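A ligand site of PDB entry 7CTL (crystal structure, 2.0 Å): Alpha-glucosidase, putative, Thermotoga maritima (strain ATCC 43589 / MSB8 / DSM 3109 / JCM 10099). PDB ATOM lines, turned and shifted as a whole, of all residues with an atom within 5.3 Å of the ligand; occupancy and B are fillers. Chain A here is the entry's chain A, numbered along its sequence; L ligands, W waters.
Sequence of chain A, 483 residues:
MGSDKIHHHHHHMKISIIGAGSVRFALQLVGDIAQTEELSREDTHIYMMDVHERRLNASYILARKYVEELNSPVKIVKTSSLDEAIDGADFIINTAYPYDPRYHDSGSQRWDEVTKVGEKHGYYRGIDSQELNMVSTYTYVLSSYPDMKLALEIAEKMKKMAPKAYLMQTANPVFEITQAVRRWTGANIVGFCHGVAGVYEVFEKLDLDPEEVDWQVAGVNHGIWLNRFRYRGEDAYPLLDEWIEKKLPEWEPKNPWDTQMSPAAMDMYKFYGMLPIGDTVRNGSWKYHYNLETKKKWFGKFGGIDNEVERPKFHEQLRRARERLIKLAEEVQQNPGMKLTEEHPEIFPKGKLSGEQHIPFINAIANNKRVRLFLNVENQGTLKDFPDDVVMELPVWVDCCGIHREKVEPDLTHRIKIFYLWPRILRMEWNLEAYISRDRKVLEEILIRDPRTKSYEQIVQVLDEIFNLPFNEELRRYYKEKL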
ATOM      1  N   ILE A  18      15.495   4.248  26.029  1.00  0.00           N
ATOM      2  CA  ILE A  18      14.970   3.230  26.916  1.00  0.00           C
ATOM      3  C   ILE A  18      13.571   2.875  26.424  1.00  0.00           C
ATOM      4  O   ILE A  18      12.718   3.755  26.299  1.00  0.00           O
ATOM      5  CB  ILE A  18      14.944   3.721  28.365  1.00  0.00           C
ATOM      6  CG1 ILE A  18      16.270   4.399  28.738  1.00  0.00           C
ATOM      7  CG2 ILE A  18      14.574   2.589  29.298  1.00  0.00           C
ATOM      8  CD1 ILE A  18      17.517   3.522  28.591  1.00  0.00           C
ATOM      9  N   GLY A  19      13.351   1.599  26.137  1.00  0.00           N
ATOM     10  CA  GLY A  19      12.169   1.174  25.411  1.00  0.00           C
ATOM     11  C   GLY A  19      12.320   1.285  23.913  1.00  0.00           C
ATOM     12  O   GLY A  19      11.347   1.606  23.215  1.00  0.00           O
ATOM     13  N   ALA A  20      13.525   1.052  23.389  1.00  0.00           N
ATOM     14  CA  ALA A  20      13.787   1.198  21.967  1.00  0.00           C
ATOM     15  C   ALA A  20      13.037   0.173  21.121  1.00  0.00           C
ATOM     16  O   ALA A  20      13.019   0.302  19.895  1.00  0.00           O
ATOM     17  CB  ALA A  20      15.297   1.121  21.722  1.00  0.00           C
ATOM     18  N   GLY A  21      12.411  -0.831  21.732  1.00  0.00           N
ATOM     19  CA  GLY A  21      11.444  -1.651  21.032  1.00  0.00           C
ATOM     20  C   GLY A  21      10.238  -0.886  20.523  1.00  0.00           C
ATOM     21  O   GLY A  21       9.433  -1.439  19.763  1.00  0.00           O
ATOM     22  N   SER A  22      10.077   0.368  20.947  1.00  0.00           N
ATOM     23  CA  SER A  22       9.068   1.252  20.374  1.00  0.00           C
ATOM     24  C   SER A  22       9.565   1.661  18.989  1.00  0.00           C
ATOM     25  O   SER A  22      10.118   2.746  18.795  1.00  0.00           O
ATOM     26  CB  SER A  22       8.824   2.457  21.270  1.00  0.00           C
ATOM     27  OG  SER A  22       7.759   3.257  20.781  1.00  0.00           O
ATOM     28  N   PHE A  25       9.040   5.095  16.887  1.00  0.00           N
ATOM     29  CA  PHE A  25       9.607   6.231  17.598  1.00  0.00           C
ATOM     30  C   PHE A  25      11.125   6.160  17.607  1.00  0.00           C
ATOM     31  O   PHE A  25      11.800   7.167  17.417  1.00  0.00           O
ATOM     32  CB  PHE A  25       9.068   6.293  19.029  1.00  0.00           C
ATOM     33  CG  PHE A  25       9.525   7.495  19.785  1.00  0.00           C
ATOM     34  CD1 PHE A  25       9.468   8.750  19.197  1.00  0.00           C
ATOM     35  CD2 PHE A  25      10.002   7.378  21.076  1.00  0.00           C
ATOM     36  CE1 PHE A  25       9.887   9.876  19.893  1.00  0.00           C
ATOM     37  CE2 PHE A  25      10.431   8.505  21.782  1.00  0.00           C
ATOM     38  CZ  PHE A  25      10.366   9.754  21.192  1.00  0.00           C
ATOM     39  N   GLN A  28      12.186   7.258  14.222  1.00  0.00           N
ATOM     40  CA  GLN A  28      12.078   8.713  14.141  1.00  0.00           C
ATOM     41  C   GLN A  28      13.287   9.378  14.790  1.00  0.00           C
ATOM     42  O   GLN A  28      13.877  10.302  14.223  1.00  0.00           O
ATOM     43  CB  GLN A  28      10.773   9.170  14.816  1.00  0.00           C
ATOM     44  CG  GLN A  28      10.476  10.663  14.713  1.00  0.00           C
ATOM     45  CD  GLN A  28       9.159  11.043  15.380  1.00  0.00           C
ATOM     46  OE1 GLN A  28       9.138  11.531  16.513  1.00  0.00           O
ATOM     47  NE2 GLN A  28       8.046  10.810  14.681  1.00  0.00           N
ATOM     48  N   MET A  49      17.959   0.255  24.161  1.00  0.00           N
ATOM     49  CA  MET A  49      17.771  -0.656  25.264  1.00  0.00           C
ATOM     50  C   MET A  49      16.294  -0.999  25.436  1.00  0.00           C
ATOM     51  O   MET A  49      15.414  -0.141  25.282  1.00  0.00           O
ATOM     52  CB  MET A  49      18.335  -0.066  26.556  1.00  0.00           C
ATOM     53  CG  MET A  49      18.295  -1.027  27.722  1.00  0.00           C
ATOM     54  SD  MET A  49      16.797  -0.760  28.680  1.00  0.00           S
ATOM     55  CE  MET A  49      16.616  -2.356  29.449  1.00  0.00           C
ATOM     56  N   ASP A  50      16.024  -2.273  25.740  1.00  0.00           N
ATOM     57  CA  ASP A  50      14.651  -2.761  25.892  1.00  0.00           C
ATOM     58  C   ASP A  50      14.714  -4.133  26.540  1.00  0.00           C
ATOM     59  O   ASP A  50      15.738  -4.831  26.442  1.00  0.00           O
ATOM     60  CB  ASP A  50      13.953  -2.815  24.519  1.00  0.00           C
ATOM     61  CG  ASP A  50      12.443  -2.847  24.614  1.00  0.00           C
ATOM     62  OD1 ASP A  50      11.908  -3.746  25.301  1.00  0.00           O
ATOM     63  OD2 ASP A  50      11.781  -1.976  24.000  1.00  0.00           O
ATOM     64  N   VAL A  51      13.628  -4.520  27.218  1.00  0.00           N
ATOM     65  CA  VAL A  51      13.540  -5.819  27.890  1.00  0.00           C
ATOM     66  C   VAL A  51      12.999  -6.905  26.963  1.00  0.00           C
ATOM     67  O   VAL A  51      13.049  -8.096  27.316  1.00  0.00           O
ATOM     68  CB  VAL A  51      12.663  -5.769  29.152  1.00  0.00           C
ATOM     69  CG1 VAL A  51      13.249  -4.790  30.157  1.00  0.00           C
ATOM     70  CG2 VAL A  51      11.210  -5.362  28.814  1.00  0.00           C
ATOM     71  N   HIS A  52      12.502  -6.538  25.794  1.00  0.00           N
ATOM     72  CA  HIS A  52      11.923  -7.460  24.832  1.00  0.00           C
ATOM     73  C   HIS A  52      12.968  -7.726  23.743  1.00  0.00           C
ATOM     74  O   HIS A  52      13.248  -6.852  22.928  1.00  0.00           O
ATOM     75  CB  HIS A  52      10.644  -6.855  24.257  1.00  0.00           C
ATOM     76  CG  HIS A  52       9.741  -7.854  23.599  1.00  0.00           C
ATOM     77  ND1 HIS A  52       9.914  -8.280  22.296  1.00  0.00           N
ATOM     78  CD2 HIS A  52       8.629  -8.484  24.052  1.00  0.00           C
ATOM     79  CE1 HIS A  52       8.965  -9.148  21.995  1.00  0.00           C
ATOM     80  NE2 HIS A  52       8.176  -9.286  23.034  1.00  0.00           N
ATOM     81  N   ARG A  55      11.635  -7.416  19.842  1.00  0.00           N
ATOM     82  CA  ARG A  55      11.397  -6.027  19.444  1.00  0.00           C
ATOM     83  C   ARG A  55      12.695  -5.227  19.417  1.00  0.00           C
ATOM     84  O   ARG A  55      12.919  -4.428  18.500  1.00  0.00           O
ATOM     85  CB  ARG A  55      10.400  -5.368  20.388  1.00  0.00           C
ATOM     86  CG  ARG A  55       8.941  -5.718  20.107  1.00  0.00           C
ATOM     87  CD  ARG A  55       8.029  -4.679  20.755  1.00  0.00           C
ATOM     88  NE  ARG A  55       8.099  -4.737  22.215  1.00  0.00           N
ATOM     89  CZ  ARG A  55       7.348  -5.530  22.964  1.00  0.00           C
ATOM     90  NH1 ARG A  55       6.450  -6.331  22.402  1.00  0.00           N
ATOM     91  NH2 ARG A  55       7.468  -5.508  24.280  1.00  0.00           N
ATOM     92  N   THR A  95      10.940   6.038  26.749  1.00  0.00           N
ATOM     93  CA  THR A  95       9.691   5.722  26.072  1.00  0.00           C
ATOM     94  C   THR A  95       9.213   4.315  26.422  1.00  0.00           C
ATOM     95  O   THR A  95       8.389   3.741  25.702  1.00  0.00           O
ATOM     96  CB  THR A  95       9.858   5.867  24.554  1.00  0.00           C
ATOM     97  OG1 THR A  95       8.583   5.700  23.891  1.00  0.00           O
ATOM     98  CG2 THR A  95      10.862   4.864  23.999  1.00  0.00           C
ATOM     99  N   ALA A  96       9.704   3.757  27.524  1.00  0.00           N
ATOM    100  CA  ALA A  96       9.354   2.397  27.905  1.00  0.00           C
ATOM    101  C   ALA A  96       7.937   2.329  28.481  1.00  0.00           C
ATOM    102  O   ALA A  96       7.455   3.268  29.110  1.00  0.00           O
ATOM    103  CB  ALA A  96      10.357   1.879  28.932  1.00  0.00           C
ATOM    104  N   TYR A  97       7.280   1.196  28.253  1.00  0.00           N
ATOM    105  CA  TYR A  97       5.924   0.959  28.746  1.00  0.00           C
ATOM    106  C   TYR A  97       5.932  -0.397  29.442  1.00  0.00           C
ATOM    107  O   TYR A  97       5.844  -1.446  28.777  1.00  0.00           O
ATOM    108  CB  TYR A  97       4.917   0.991  27.593  1.00  0.00           C
ATOM    109  CG  TYR A  97       3.456   1.157  27.975  1.00  0.00           C
ATOM    110  CD1 TYR A  97       3.083   1.658  29.221  1.00  0.00           C
ATOM    111  CD2 TYR A  97       2.447   0.818  27.076  1.00  0.00           C
ATOM    112  CE1 TYR A  97       1.742   1.811  29.551  1.00  0.00           C
ATOM    113  CE2 TYR A  97       1.106   0.971  27.406  1.00  0.00           C
ATOM    114  CZ  TYR A  97       0.760   1.461  28.639  1.00  0.00           C
ATOM    115  OH  TYR A  97      -0.555   1.603  28.955  1.00  0.00           O
ATOM    116  N   PRO A  98       6.092  -0.423  30.766  1.00  0.00           N
ATOM    117  CA  PRO A  98       6.298  -1.695  31.460  1.00  0.00           C
ATOM    118  C   PRO A  98       5.133  -2.664  31.335  1.00  0.00           C
ATOM    119  O   PRO A  98       3.984  -2.290  31.077  1.00  0.00           O
ATOM    120  CB  PRO A  98       6.496  -1.263  32.920  1.00  0.00           C
ATOM    121  CG  PRO A  98       7.052   0.085  32.826  1.00  0.00           C
ATOM    122  CD  PRO A  98       6.336   0.721  31.651  1.00  0.00           C
ATOM    123  N   TYR A  99       5.458  -3.939  31.540  1.00  0.00           N
ATOM    124  CA  TYR A  99       4.449  -4.990  31.504  1.00  0.00           C
ATOM    125  C   TYR A  99       4.986  -6.195  32.259  1.00  0.00           C
ATOM    126  O   TYR A  99       6.196  -6.306  32.493  1.00  0.00           O
ATOM    127  CB  TYR A  99       4.073  -5.380  30.068  1.00  0.00           C
ATOM    128  CG  TYR A  99       5.236  -5.970  29.290  1.00  0.00           C
ATOM    129  CD1 TYR A  99       5.377  -7.350  29.155  1.00  0.00           C
ATOM    130  CD2 TYR A  99       6.183  -5.140  28.703  1.00  0.00           C
ATOM    131  CE1 TYR A  99       6.459  -7.895  28.438  1.00  0.00           C
ATOM    132  CE2 TYR A  99       7.259  -5.667  27.999  1.00  0.00           C
ATOM    133  CZ  TYR A  99       7.394  -7.041  27.869  1.00  0.00           C
ATOM    134  OH  TYR A  99       8.450  -7.541  27.150  1.00  0.00           O
ATOM    135  N   SER A 106       3.137  -6.685  25.832  1.00  0.00           N
ATOM    136  CA  SER A 106       3.385  -5.255  25.810  1.00  0.00           C
ATOM    137  C   SER A 106       2.469  -4.586  26.823  1.00  0.00           C
ATOM    138  O   SER A 106       1.540  -5.198  27.346  1.00  0.00           O
ATOM    139  CB  SER A 106       3.185  -4.674  24.404  1.00  0.00           C
ATOM    140  OG  SER A 106       1.815  -4.539  24.082  1.00  0.00           O
ATOM    141  N   GLY A 107       2.732  -3.303  27.079  1.00  0.00           N
ATOM    142  CA  GLY A 107       2.041  -2.603  28.159  1.00  0.00           C
ATOM    143  C   GLY A 107       0.588  -2.257  27.869  1.00  0.00           C
ATOM    144  O   GLY A 107      -0.203  -2.083  28.810  1.00  0.00           O
ATOM    145  N   SER A 108       0.223  -2.090  26.602  1.00  0.00           N
ATOM    146  CA  SER A 108      -1.167  -1.742  26.271  1.00  0.00           C
ATOM    147  C   SER A 108      -2.165  -2.744  26.851  1.00  0.00           C
ATOM    148  O   SER A 108      -3.300  -2.375  27.174  1.00  0.00           O
ATOM    149  CB  SER A 108      -1.353  -1.673  24.753  1.00  0.00           C
ATOM    150  OG  SER A 108      -1.050  -2.929  24.158  1.00  0.00           O
ATOM    151  N   THR A 137      -4.839   5.461  28.186  1.00  0.00           N
ATOM    152  CA  THR A 137      -3.543   4.943  28.666  1.00  0.00           C
ATOM    153  C   THR A 137      -2.679   5.994  29.354  1.00  0.00           C
ATOM    154  O   THR A 137      -1.497   5.752  29.564  1.00  0.00           O
ATOM    155  CB  THR A 137      -2.709   4.291  27.554  1.00  0.00           C
ATOM    156  OG1 THR A 137      -2.156   5.284  26.691  1.00  0.00           O
ATOM    157  CG2 THR A 137      -3.554   3.295  26.714  1.00  0.00           C
ATOM    158  N   LEU A 150       9.361   2.766  37.259  1.00  0.00           N
ATOM    159  CA  LEU A 150      10.474   2.701  36.322  1.00  0.00           C
ATOM    160  C   LEU A 150      11.153   4.072  36.198  1.00  0.00           C
ATOM    161  O   LEU A 150      12.385   4.161  36.200  1.00  0.00           O
ATOM    162  CB  LEU A 150       9.991   2.210  34.962  1.00  0.00           C
ATOM    163  CG  LEU A 150      11.058   2.213  33.874  1.00  0.00           C
ATOM    164  CD1 LEU A 150      12.230   1.314  34.239  1.00  0.00           C
ATOM    165  CD2 LEU A 150      10.458   1.771  32.587  1.00  0.00           C
ATOM    166  N   THR A 170       9.108  10.681  27.921  1.00  0.00           N
ATOM    167  CA  THR A 170       8.003  10.686  26.968  1.00  0.00           C
ATOM    168  C   THR A 170       6.885   9.707  27.317  1.00  0.00           C
ATOM    169  O   THR A 170       5.779   9.863  26.794  1.00  0.00           O
ATOM    170  CB  THR A 170       8.475  10.325  25.553  1.00  0.00           C
ATOM    171  OG1 THR A 170       8.814   8.936  25.516  1.00  0.00           O
ATOM    172  CG2 THR A 170       9.679  11.157  25.163  1.00  0.00           C
ATOM    173  N   ALA A 171       7.140   8.728  28.190  1.00  0.00           N
ATOM    174  CA  ALA A 171       6.128   7.765  28.593  1.00  0.00           C
ATOM    175  C   ALA A 171       5.163   8.406  29.577  1.00  0.00           C
ATOM    176  O   ALA A 171       5.568   9.144  30.473  1.00  0.00           O
ATOM    177  CB  ALA A 171       6.784   6.537  29.230  1.00  0.00           C
ATOM    178  N   ASN A 172       3.923   8.104  29.435  1.00  0.00           N
ATOM    179  CA  ASN A 172       2.858   8.713  30.235  1.00  0.00           C
ATOM    180  C   ASN A 172       2.640   7.971  31.558  1.00  0.00           C
ATOM    181  O   ASN A 172       2.883   6.764  31.646  1.00  0.00           O
ATOM    182  CB  ASN A 172       1.553   8.728  29.450  1.00  0.00           C
ATOM    183  CG  ASN A 172       1.506   9.863  28.449  1.00  0.00           C
ATOM    184  OD1 ASN A 172       1.904  10.994  28.746  1.00  0.00           O
ATOM    185  ND2 ASN A 172       1.047   9.563  27.235  1.00  0.00           N
ATOM    186  N   PHE A 192       8.185  15.614  27.765  1.00  0.00           N
ATOM    187  CA  PHE A 192       8.083  15.886  26.336  1.00  0.00           C
ATOM    188  C   PHE A 192       6.727  15.450  25.795  1.00  0.00           C
ATOM    189  O   PHE A 192       6.322  14.287  25.986  1.00  0.00           O
ATOM    190  CB  PHE A 192       9.184  15.169  25.545  1.00  0.00           C
ATOM    191  CG  PHE A 192      10.523  15.840  25.634  1.00  0.00           C
ATOM    192  CD1 PHE A 192      11.261  15.755  26.803  1.00  0.00           C
ATOM    193  CD2 PHE A 192      11.028  16.549  24.562  1.00  0.00           C
ATOM    194  CE1 PHE A 192      12.489  16.379  26.905  1.00  0.00           C
ATOM    195  CE2 PHE A 192      12.260  17.171  24.650  1.00  0.00           C
ATOM    196  CZ  PHE A 192      12.986  17.081  25.831  1.00  0.00           C
ATOM    197  N   CYS A 193       6.039  16.372  25.111  1.00  0.00           N
ATOM    198  CA  CYS A 193       4.821  16.105  24.359  1.00  0.00           C
ATOM    199  C   CYS A 193       4.622  17.209  23.320  1.00  0.00           C
ATOM    200  O   CYS A 193       4.765  18.394  23.633  1.00  0.00           O
ATOM    201  CB  CYS A 193       3.596  16.034  25.291  1.00  0.00           C
ATOM    202  SG  CYS A 193       1.965  16.081  24.457  1.00  0.00           S
ATOM    203  N   HIS A 194       4.271  16.822  22.084  1.00  0.00           N
ATOM    204  CA  HIS A 194       4.084  17.785  21.004  1.00  0.00           C
ATOM    205  C   HIS A 194       2.606  18.059  20.687  1.00  0.00           C
ATOM    206  O   HIS A 194       2.270  18.316  19.528  1.00  0.00           O
ATOM    207  CB  HIS A 194       4.806  17.324  19.737  1.00  0.00           C
ATOM    208  CG  HIS A 194       5.171  18.445  18.810  1.00  0.00           C
ATOM    209  ND1 HIS A 194       5.280  18.283  17.445  1.00  0.00           N
ATOM    210  CD2 HIS A 194       5.460  19.746  19.058  1.00  0.00           C
ATOM    211  CE1 HIS A 194       5.628  19.435  16.889  1.00  0.00           C
ATOM    212  NE2 HIS A 194       5.748  20.343  17.845  1.00  0.00           N
ATOM    213  N   LEU A 318      -1.844  -1.043  16.149  1.00  0.00           N
ATOM    214  CA  LEU A 318      -0.472  -0.986  16.648  1.00  0.00           C
ATOM    215  C   LEU A 318       0.131  -2.378  16.743  1.00  0.00           C
ATOM    216  O   LEU A 318       1.327  -2.553  16.473  1.00  0.00           O
ATOM    217  CB  LEU A 318      -0.432  -0.298  18.018  1.00  0.00           C
ATOM    218  CG  LEU A 318      -0.725   1.202  18.027  1.00  0.00           C
ATOM    219  CD1 LEU A 318      -0.648   1.735  19.461  1.00  0.00           C
ATOM    220  CD2 LEU A 318       0.210   1.962  17.100  1.00  0.00           C
ATOM    221  N   ARG A 322       3.478  -3.479  14.903  1.00  0.00           N
ATOM    222  CA  ARG A 322       4.601  -4.085  15.615  1.00  0.00           C
ATOM    223  C   ARG A 322       5.077  -5.353  14.918  1.00  0.00           C
ATOM    224  O   ARG A 322       6.273  -5.539  14.679  1.00  0.00           O
ATOM    225  CB  ARG A 322       4.213  -4.372  17.057  1.00  0.00           C
ATOM    226  CG  ARG A 322       5.249  -5.140  17.862  1.00  0.00           C
ATOM    227  CD  ARG A 322       4.778  -5.422  19.294  1.00  0.00           C
ATOM    228  NE  ARG A 322       4.592  -4.186  20.073  1.00  0.00           N
ATOM    229  CZ  ARG A 322       3.408  -3.647  20.381  1.00  0.00           C
ATOM    230  NH1 ARG A 322       2.264  -4.220  20.000  1.00  0.00           N
ATOM    231  NH2 ARG A 322       3.369  -2.533  21.108  1.00  0.00           N
ATOM    232  N   GLU A 356       9.267  16.388  15.490  1.00  0.00           N
ATOM    233  CA  GLU A 356       9.200  16.228  16.936  1.00  0.00           C
ATOM    234  C   GLU A 356      10.318  17.027  17.594  1.00  0.00           C
ATOM    235  O   GLU A 356      11.226  17.535  16.930  1.00  0.00           O
ATOM    236  CB  GLU A 356       9.273  14.751  17.325  1.00  0.00           C
ATOM    237  CG  GLU A 356       7.904  14.120  17.677  1.00  0.00           C
ATOM    238  CD  GLU A 356       7.345  14.604  19.022  1.00  0.00           C
ATOM    239  OE1 GLU A 356       7.822  15.613  19.571  1.00  0.00           O
ATOM    240  OE2 GLU A 356       6.425  13.934  19.543  1.00  0.00           O
ATOM    241  N   HIS A 358      12.408  16.095  20.313  1.00  0.00           N
ATOM    242  CA  HIS A 358      13.467  15.436  21.083  1.00  0.00           C
ATOM    243  C   HIS A 358      14.854  15.765  20.529  1.00  0.00           C
ATOM    244  O   HIS A 358      15.757  16.127  21.291  1.00  0.00           O
ATOM    245  CB  HIS A 358      13.220  13.930  21.094  1.00  0.00           C
ATOM    246  CG  HIS A 358      11.845  13.572  21.543  1.00  0.00           C
ATOM    247  ND1 HIS A 358      10.758  13.603  20.698  1.00  0.00           N
ATOM    248  CD2 HIS A 358      11.363  13.229  22.759  1.00  0.00           C
ATOM    249  CE1 HIS A 358       9.667  13.286  21.372  1.00  0.00           C
ATOM    250  NE2 HIS A 358      10.011  13.053  22.628  1.00  0.00           N
HETATM  251  P1  LIG L   1       5.167   0.158  23.401  1.00  0.00           P
HETATM  252  O1  LIG L   1       4.639  -0.936  24.292  1.00  0.00           O
HETATM  253  O2  LIG L   1       5.025  -0.120  21.935  1.00  0.00           O
HETATM  254  O3  LIG L   1       6.728   0.505  23.714  1.00  0.00           O
HETATM  255  C1  LIG L   1       7.160   0.269  25.004  1.00  0.00           C
HETATM  256  C2  LIG L   1       8.565  -0.337  24.848  1.00  0.00           C
HETATM  257  O4  LIG L   1       9.113  -0.237  26.025  1.00  0.00           O
HETATM  258  C3  LIG L   1       8.400  -1.837  24.529  1.00  0.00           C
HETATM  259  O5  LIG L   1       9.274  -2.303  23.568  1.00  0.00           O
HETATM  260  C4  LIG L   1       8.697  -2.472  25.901  1.00  0.00           C
HETATM  261  O6  LIG L   1       9.233  -3.829  25.627  1.00  0.00           O
HETATM  262  C5  LIG L   1       9.604  -1.689  26.437  1.00  0.00           C
HETATM  263  N1  LIG L   1       9.751  -1.796  27.871  1.00  0.00           N
HETATM  264  C6  LIG L   1       8.865  -2.187  28.781  1.00  0.00           C
HETATM  265  N2  LIG L   1       9.438  -2.171  29.985  1.00  0.00           N
HETATM  266  C7  LIG L   1      10.700  -1.767  29.811  1.00  0.00           C
HETATM  267  C8  LIG L   1      11.718  -1.566  30.719  1.00  0.00           C
HETATM  268  N3  LIG L   1      11.775  -1.730  32.166  1.00  0.00           N
HETATM  269  N4  LIG L   1      12.906  -1.156  30.293  1.00  0.00           N
HETATM  270  C9  LIG L   1      13.116  -0.907  28.983  1.00  0.00           C
HETATM  271  N5  LIG L   1      12.115  -1.099  28.087  1.00  0.00           N
HETATM  272  C10 LIG L   1      10.907  -1.534  28.516  1.00  0.00           C
HETATM  273  O7  LIG L   1       4.319   1.519  23.772  1.00  0.00           O
HETATM  274  P2  LIG L   1       4.509   2.946  23.007  1.00  0.00           P
HETATM  275  O8  LIG L   1       3.639   2.996  21.791  1.00  0.00           O
HETATM  276  O9  LIG L   1       5.941   3.193  22.656  1.00  0.00           O
HETATM  277  O10 LIG L   1       4.103   4.069  24.125  1.00  0.00           O
HETATM  278  C11 LIG L   1       4.792   4.025  25.344  1.00  0.00           C
HETATM  279  C12 LIG L   1       4.623   5.376  26.094  1.00  0.00           C
HETATM  280  O11 LIG L   1       5.478   6.230  25.618  1.00  0.00           O
HETATM  281  C13 LIG L   1       3.218   5.958  25.814  1.00  0.00           C
HETATM  282  O12 LIG L   1       2.727   6.575  26.922  1.00  0.00           O
HETATM  283  C14 LIG L   1       3.446   6.937  24.645  1.00  0.00           C
HETATM  284  O13 LIG L   1       2.470   8.068  24.670  1.00  0.00           O
HETATM  285  C15 LIG L   1       4.661   7.392  24.839  1.00  0.00           C
HETATM  286  N6  LIG L   1       5.300   7.679  23.570  1.00  0.00           N
HETATM  287  C16 LIG L   1       5.347   9.054  23.111  1.00  0.00           C
HETATM  288  C17 LIG L   1       5.884   9.401  21.727  1.00  0.00           C
HETATM  289  C18 LIG L   1       6.213  10.863  21.402  1.00  0.00           C
HETATM  290  O14 LIG L   1       6.710  11.120  20.357  1.00  0.00           O
HETATM  291  N7  LIG L   1       5.938  11.930  22.355  1.00  0.00           N
HETATM  292  C19 LIG L   1       6.399   8.311  20.804  1.00  0.00           C
HETATM  293  C20 LIG L   1       6.205   6.876  21.302  1.00  0.00           C
HETATM  294  C21 LIG L   1       5.893   6.619  22.766  1.00  0.00           C
HETATM  295  O   HOH W   1       4.754  12.046  25.540  1.00  0.00           O
HETATM  296  O   HOH W   2       9.359  -2.374  34.123  1.00  0.00           O
HETATM  297  O   HOH W   3       8.537  -4.229  31.984  1.00  0.00           O
HETATM  298  O   HOH W   4       1.836  -1.415  24.205  1.00  0.00           O
HETATM  299  O   HOH W   5       5.333  -2.343  26.347  1.00  0.00           O
HETATM  300  O   HOH W   6      13.607  -1.777  34.593  1.00  0.00           O
HETATM  301  O   HOH W   7       0.930   5.076  28.480  1.00  0.00           O
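OD2 of Asp 50 is in hydrogen-bond range of O5 of the ligand.
OG of Ser 22 lies within hydrogen-bond range of O9 of the ligand (2.6 Å).
The guanidinium group (NH2) of Arg 55 is in hydrogen-bond range of an oxygen (O6) of the ligand (2.8 Å).
A nitrogen (N7) of the ligand lies within hydrogen-bond range of the side-chain carboxylate of Glu 356 (3.5 Å).
O2 of the ligand is in salt-bridge range of NH2 of Arg 322.
The backbone NH (N) of Tyr 97 lies within hydrogen-bond range of an oxygen (O4) of the ligand, at 3.2 Å.
The backbone NH of Asn 172 sits at hydrogen-bond distance from an oxygen (O12) of the ligand, 3.2 Å away.
The side-chain amide nitrogen (ND2) of Asn 172 lies within hydrogen-bond range of an oxygen (O13) of the ligand.
OD2 of Asp 50 is in hydrogen-bond range of N of Gly 21, 2.6 Å away.
The side-chain carboxylate of Asp 50 is in hydrogen-bond range of the backbone NH of His 52, 2.9 Å away.
N of Arg 55 is in hydrogen-bond range of ND1 of His 52 (3.1 Å).
The backbone carbonyl oxygen (O) of Ile 18 sits at hydrogen-bond distance from the backbone NH (N) of Thr 95 (2.9 Å).
The backbone NH of Ala 96 is in hydrogen-bond range of the backbone carbonyl oxygen of Ile 18, at 3.3 Å.
The backbone NH of Gly 19 is in hydrogen-bond range of the backbone carbonyl oxygen of Met 49, at 2.8 Å.
The backbone carbonyl oxygen of Met 49 lies within hydrogen-bond range of the backbone NH of Ala 20 (2.9 Å).
Ile 18 touches the ligand.
CA of Gly 19 touches O4 of the ligand, 3.4 Å away.
CA of Gly 21 touches O5 of the ligand, 3.4 Å away.
CG of Phe 25 touches C19 of the ligand (3.4 Å).
Met 49 touches the ligand (SD to C9, 3.7 Å).
Val 51 touches the ligand (CG1 to C8, 3.6 Å).
His 52 touches the ligand (CB to O6, 3.6 Å).
OG1 of Thr 95 touches C21 of the ligand, 3.1 Å away.
CA of Ala 96 touches O4 of the ligand, at 3.2 Å.
Pro 98 touches the ligand (CA to N2, 3.5 Å).
CE2 of Tyr 99 touches O6 of the ligand, at 3.6 Å.
CD1 of Leu 150 touches N3 of the ligand, 3.7 Å away.
Thr 170 touches the ligand.
CA of Ala 171 touches O11 of the ligand, 3.4 Å away.
His 358 touches the ligand (CE1 to O14, 3.8 Å).
Hydrophobic or aromatic side chains that line the ligand: Ile 18, Phe 25, Met 49, Val 51, His 52, Ala 96, Tyr 97, Tyr 99, Leu 150, Ala 171 and His 358.
Of the 32 residues printed, 22 come within 4 Å of the ligand.
Water W5 lies within hydrogen-bond range of O1 of the ligand (2.6 Å), O of Tyr 97 (2.6 Å) and N of Gly 107 (2.9 Å).
Water W7 lies within hydrogen-bond range of the backbone carbonyl oxygen of Thr 137 (2.7 Å) and an oxygen (O12) of the ligand (2.8 Å).
Water W4 lies within hydrogen-bond range of O1 of the ligand, N of Ser 108 and OG of Ser 106.
Water W3 bridges a nitrogen (N2) of the ligand (3.0 Å) and the backbone NH (N) of Tyr 99 (3.1 Å).
Water W1 lies within hydrogen-bond range of the backbone carbonyl oxygen (O) of Thr 170 (2.7 Å), the backbone carbonyl oxygen (O) of Phe 192 (2.8 Å) and a nitrogen (N7) of the ligand (3.4 Å).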
